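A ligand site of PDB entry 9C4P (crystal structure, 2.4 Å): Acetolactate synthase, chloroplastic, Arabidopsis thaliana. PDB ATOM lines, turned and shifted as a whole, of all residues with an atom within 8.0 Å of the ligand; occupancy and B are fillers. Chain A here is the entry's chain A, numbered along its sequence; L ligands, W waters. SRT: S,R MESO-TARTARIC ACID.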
ATOM      1  N   GLY A  26     -36.571  17.985  25.643  1.00  0.00           N
ATOM      2  CA  GLY A  26     -36.491  16.635  26.168  1.00  0.00           C
ATOM      3  C   GLY A  26     -35.078  16.098  26.319  1.00  0.00           C
ATOM      4  O   GLY A  26     -34.912  14.892  26.521  1.00  0.00           O
ATOM      5  N   VAL A  27     -34.066  16.952  26.210  1.00  0.00           N
ATOM      6  CA  VAL A  27     -32.686  16.517  26.333  1.00  0.00           C
ATOM      7  C   VAL A  27     -32.438  16.030  27.756  1.00  0.00           C
ATOM      8  O   VAL A  27     -32.767  16.713  28.730  1.00  0.00           O
ATOM      9  CB  VAL A  27     -31.718  17.649  25.956  1.00  0.00           C
ATOM     10  CG1 VAL A  27     -30.272  17.243  26.244  1.00  0.00           C
ATOM     11  CG2 VAL A  27     -31.893  18.020  24.489  1.00  0.00           C
ATOM     12  N   GLU A  28     -31.847  14.840  27.878  1.00  0.00           N
ATOM     13  CA  GLU A  28     -31.430  14.298  29.162  1.00  0.00           C
ATOM     14  C   GLU A  28     -29.934  14.126  29.298  1.00  0.00           C
ATOM     15  O   GLU A  28     -29.426  14.118  30.421  1.00  0.00           O
ATOM     16  CB  GLU A  28     -32.109  12.942  29.408  1.00  0.00           C
ATOM     17  CG  GLU A  28     -33.611  13.004  29.469  1.00  0.00           C
ATOM     18  CD  GLU A  28     -34.240  11.622  29.535  1.00  0.00           C
ATOM     19  OE1 GLU A  28     -34.202  10.909  28.514  1.00  0.00           O
ATOM     20  OE2 GLU A  28     -34.751  11.249  30.613  1.00  0.00           O
ATOM     21  N   THR A  29     -29.209  13.988  28.191  1.00  0.00           N
ATOM     22  CA  THR A  29     -27.777  13.739  28.224  1.00  0.00           C
ATOM     23  C   THR A  29     -27.087  14.629  27.200  1.00  0.00           C
ATOM     24  O   THR A  29     -27.537  14.726  26.056  1.00  0.00           O
ATOM     25  CB  THR A  29     -27.466  12.266  27.926  1.00  0.00           C
ATOM     26  OG1 THR A  29     -28.214  11.429  28.807  1.00  0.00           O
ATOM     27  CG2 THR A  29     -25.980  11.990  28.113  1.00  0.00           C
ATOM     28  N   SER A  50     -32.345  17.785  35.344  1.00  0.00           N
ATOM     29  CA  SER A  50     -32.820  16.800  34.383  1.00  0.00           C
ATOM     30  C   SER A  50     -31.794  16.460  33.306  1.00  0.00           C
ATOM     31  O   SER A  50     -31.974  15.467  32.600  1.00  0.00           O
ATOM     32  CB  SER A  50     -34.103  17.300  33.704  1.00  0.00           C
ATOM     33  OG  SER A  50     -33.885  18.496  32.980  1.00  0.00           O
ATOM     34  N   ARG A  52     -27.906  15.403  32.361  1.00  0.00           N
ATOM     35  CA  ARG A  52     -26.644  14.843  32.826  1.00  0.00           C
ATOM     36  C   ARG A  52     -25.576  15.083  31.780  1.00  0.00           C
ATOM     37  O   ARG A  52     -25.810  14.912  30.577  1.00  0.00           O
ATOM     38  CB  ARG A  52     -26.808  13.340  33.093  1.00  0.00           C
ATOM     39  CG  ARG A  52     -25.507  12.545  33.156  1.00  0.00           C
ATOM     40  CD  ARG A  52     -25.784  11.052  32.954  1.00  0.00           C
ATOM     41  NE  ARG A  52     -24.584  10.234  33.102  1.00  0.00           N
ATOM     42  CZ  ARG A  52     -24.539   8.928  32.865  1.00  0.00           C
ATOM     43  NH1 ARG A  52     -25.613   8.258  32.466  1.00  0.00           N
ATOM     44  NH2 ARG A  52     -23.394   8.277  33.037  1.00  0.00           N
ATOM     45  N   VAL A  54     -21.911  13.917  30.314  1.00  0.00           N
ATOM     46  CA  VAL A  54     -20.860  12.917  30.234  1.00  0.00           C
ATOM     47  C   VAL A  54     -19.622  13.620  29.706  1.00  0.00           C
ATOM     48  O   VAL A  54     -19.541  13.957  28.529  1.00  0.00           O
ATOM     49  CB  VAL A  54     -21.268  11.736  29.339  1.00  0.00           C
ATOM     50  CG1 VAL A  54     -20.111  10.757  29.199  1.00  0.00           C
ATOM     51  CG2 VAL A  54     -22.488  11.027  29.930  1.00  0.00           C
ATOM     52  N   TYR A  69     -25.000   7.860  20.753  1.00  0.00           N
ATOM     53  CA  TYR A  69     -26.258   8.137  21.431  1.00  0.00           C
ATOM     54  C   TYR A  69     -27.403   8.241  20.434  1.00  0.00           C
ATOM     55  O   TYR A  69     -28.458   7.622  20.612  1.00  0.00           O
ATOM     56  CB  TYR A  69     -26.111   9.427  22.239  1.00  0.00           C
ATOM     57  CG  TYR A  69     -27.285   9.794  23.129  1.00  0.00           C
ATOM     58  CD1 TYR A  69     -28.376  10.502  22.635  1.00  0.00           C
ATOM     59  CD2 TYR A  69     -27.275   9.457  24.480  1.00  0.00           C
ATOM     60  CE1 TYR A  69     -29.445  10.842  23.449  1.00  0.00           C
ATOM     61  CE2 TYR A  69     -28.342   9.804  25.307  1.00  0.00           C
ATOM     62  CZ  TYR A  69     -29.413  10.493  24.786  1.00  0.00           C
ATOM     63  OH  TYR A  69     -30.470  10.833  25.606  1.00  0.00           O
ATOM     64  N   SER A  72     -28.133   4.905  18.195  1.00  0.00           N
ATOM     65  CA  SER A  72     -28.665   3.778  18.948  1.00  0.00           C
ATOM     66  C   SER A  72     -30.035   4.058  19.565  1.00  0.00           C
ATOM     67  O   SER A  72     -30.610   3.150  20.164  1.00  0.00           O
ATOM     68  CB  SER A  72     -27.693   3.384  20.058  1.00  0.00           C
ATOM     69  OG  SER A  72     -27.725   4.313  21.125  1.00  0.00           O
ATOM     70  N   SER A  73     -30.561   5.274  19.420  1.00  0.00           N
ATOM     71  CA  SER A  73     -31.797   5.643  20.106  1.00  0.00           C
ATOM     72  C   SER A  73     -32.826   6.322  19.217  1.00  0.00           C
ATOM     73  O   SER A  73     -34.009   6.329  19.584  1.00  0.00           O
ATOM     74  CB  SER A  73     -31.497   6.577  21.280  1.00  0.00           C
ATOM     75  OG  SER A  73     -31.113   7.859  20.827  1.00  0.00           O
ATOM     76  N   LYS A  75     -33.002   9.466  18.942  1.00  0.00           N
ATOM     77  CA  LYS A  75     -33.029  10.808  19.499  1.00  0.00           C
ATOM     78  C   LYS A  75     -31.809  11.593  19.015  1.00  0.00           C
ATOM     79  O   LYS A  75     -30.808  10.997  18.598  1.00  0.00           O
ATOM     80  CB  LYS A  75     -33.030  10.741  21.025  1.00  0.00           C
ATOM     81  CG  LYS A  75     -34.182   9.956  21.616  1.00  0.00           C
ATOM     82  CD  LYS A  75     -34.227  10.072  23.140  1.00  0.00           C
ATOM     83  CE  LYS A  75     -32.987   9.467  23.790  1.00  0.00           C
ATOM     84  NZ  LYS A  75     -33.064   9.501  25.280  1.00  0.00           N
ATOM     85  N   GLY A 437     -21.790   6.493  23.979  1.00  0.00           N
ATOM     86  CA  GLY A 437     -23.084   7.128  23.793  1.00  0.00           C
ATOM     87  C   GLY A 437     -24.222   6.129  23.731  1.00  0.00           C
ATOM     88  O   GLY A 437     -25.315   6.381  24.250  1.00  0.00           O
ATOM     89  N   ALA A 438     -23.984   4.983  23.090  1.00  0.00           N
ATOM     90  CA  ALA A 438     -25.019   3.946  23.005  1.00  0.00           C
ATOM     91  C   ALA A 438     -25.343   3.381  24.381  1.00  0.00           C
ATOM     92  O   ALA A 438     -26.510   3.103  24.683  1.00  0.00           O
ATOM     93  CB  ALA A 438     -24.581   2.830  22.061  1.00  0.00           C
ATOM     94  N   SER A 439     -24.323   3.195  25.224  1.00  0.00           N
ATOM     95  CA  SER A 439     -24.562   2.649  26.552  1.00  0.00           C
ATOM     96  C   SER A 439     -25.308   3.644  27.432  1.00  0.00           C
ATOM     97  O   SER A 439     -26.202   3.247  28.190  1.00  0.00           O
ATOM     98  CB  SER A 439     -23.231   2.253  27.197  1.00  0.00           C
ATOM     99  OG  SER A 439     -23.436   1.697  28.484  1.00  0.00           O
ATOM    100  N   VAL A 440     -24.960   4.929  27.350  1.00  0.00           N
ATOM    101  CA  VAL A 440     -25.694   5.941  28.116  1.00  0.00           C
ATOM    102  C   VAL A 440     -27.151   5.991  27.668  1.00  0.00           C
ATOM    103  O   VAL A 440     -28.061   6.143  28.481  1.00  0.00           O
ATOM    104  CB  VAL A 440     -25.001   7.316  27.979  1.00  0.00           C
ATOM    105  CG1 VAL A 440     -25.861   8.407  28.618  1.00  0.00           C
ATOM    106  CG2 VAL A 440     -23.627   7.290  28.612  1.00  0.00           C
ATOM    107  N   ALA A 441     -27.393   5.850  26.364  1.00  0.00           N
ATOM    108  CA  ALA A 441     -28.757   5.866  25.844  1.00  0.00           C
ATOM    109  C   ALA A 441     -29.500   4.562  26.131  1.00  0.00           C
ATOM    110  O   ALA A 441     -30.730   4.575  26.257  1.00  0.00           O
ATOM    111  CB  ALA A 441     -28.751   6.144  24.352  1.00  0.00           C
ATOM    112  N   ASN A 442     -28.779   3.446  26.242  1.00  0.00           N
ATOM    113  CA  ASN A 442     -29.376   2.129  26.462  1.00  0.00           C
ATOM    114  C   ASN A 442     -28.654   1.449  27.618  1.00  0.00           C
ATOM    115  O   ASN A 442     -27.875   0.510  27.420  1.00  0.00           O
ATOM    116  CB  ASN A 442     -29.307   1.281  25.199  1.00  0.00           C
ATOM    117  CG  ASN A 442     -29.894   1.998  23.986  1.00  0.00           C
ATOM    118  OD1 ASN A 442     -31.079   1.891  23.701  1.00  0.00           O
ATOM    119  ND2 ASN A 442     -29.045   2.730  23.273  1.00  0.00           N
ATOM    120  N   PRO A 443     -28.905   1.883  28.858  1.00  0.00           N
ATOM    121  CA  PRO A 443     -28.085   1.427  29.993  1.00  0.00           C
ATOM    122  C   PRO A 443     -28.301  -0.036  30.361  1.00  0.00           C
ATOM    123  O   PRO A 443     -27.494  -0.582  31.128  1.00  0.00           O
ATOM    124  CB  PRO A 443     -28.504   2.357  31.126  1.00  0.00           C
ATOM    125  CG  PRO A 443     -29.896   2.782  30.787  1.00  0.00           C
ATOM    126  CD  PRO A 443     -29.972   2.825  29.279  1.00  0.00           C
ATOM    127  N   LEU A 471     -19.752   2.701  32.815  1.00  0.00           N
ATOM    128  CA  LEU A 471     -20.530   2.193  31.684  1.00  0.00           C
ATOM    129  C   LEU A 471     -20.084   0.768  31.365  1.00  0.00           C
ATOM    130  O   LEU A 471     -18.890   0.504  31.254  1.00  0.00           O
ATOM    131  CB  LEU A 471     -20.335   3.083  30.468  1.00  0.00           C
ATOM    132  CG  LEU A 471     -20.677   4.564  30.664  1.00  0.00           C
ATOM    133  CD1 LEU A 471     -20.306   5.373  29.433  1.00  0.00           C
ATOM    134  CD2 LEU A 471     -22.154   4.724  31.000  1.00  0.00           C
HETATM  135  O1  SRT L   1     -33.201   6.447  28.973  1.00  0.00           O
HETATM  136  O11 SRT L   1     -32.694   6.370  26.858  1.00  0.00           O
HETATM  137  C1  SRT L   1     -32.400   6.700  28.038  1.00  0.00           C
HETATM  138  C2  SRT L   1     -31.072   7.399  28.323  1.00  0.00           C
HETATM  139  O2  SRT L   1     -31.106   8.736  27.884  1.00  0.00           O
HETATM  140  C3  SRT L   1     -30.774   7.362  29.823  1.00  0.00           C
HETATM  141  O3  SRT L   1     -29.414   7.592  30.034  1.00  0.00           O
HETATM  142  C4  SRT L   1     -31.586   8.431  30.559  1.00  0.00           C
HETATM  143  O4  SRT L   1     -32.366   9.180  29.912  1.00  0.00           O
HETATM  144  O41 SRT L   1     -31.462   8.568  31.798  1.00  0.00           O
HETATM  145  O   HOH W   1     -27.585   6.072  31.404  1.00  0.00           O
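An oxygen (O3) of the ligand sits at hydrogen-bond distance from the backbone carbonyl oxygen (O) of Val 440 (2.5 Å).
O of Ala 441 sits close to O11 of the ligand.
An oxygen (O4) of the ligand sits close to the side-chain carboxylate (OE1) of Glu 28, 2.9 Å away.
An oxygen (O2) of the ligand sits at hydrogen-bond distance from the side-chain hydroxyl of Tyr 69.
The side-chain amino group (NZ) of Lys 75 lies within salt-bridge range of an oxygen (O11) of the ligand (3.5 Å).
NZ of Lys 75 is in salt-bridge range of OE1 of Glu 28 (3.7 Å).
The backbone carbonyl oxygen (O) of Glu 28 sits at hydrogen-bond distance from the backbone NH (N) of Arg 52 (2.8 Å).
The side-chain hydroxyl (OH) of Tyr 69 lies within hydrogen-bond range of the side-chain amino group (NZ) of Lys 75.
The side-chain hydroxyl of Ser 73 is in hydrogen-bond range of the backbone carbonyl oxygen of Tyr 69 (2.7 Å).
The side-chain hydroxyl (OG) of Ser 72 sits at hydrogen-bond distance from the backbone carbonyl oxygen (O) of Tyr 69 (3.4 Å).
The side-chain hydroxyl (OG) of Ser 73 sits at hydrogen-bond distance from the backbone NH (N) of Lys 75 (3.1 Å).
The nearest printed residue that does not touch the ligand is Thr 29 (4.1 Å).
Water W1 lies within hydrogen-bond range of O3 of the ligand, O of Val 440 and NH1 of Arg 52.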
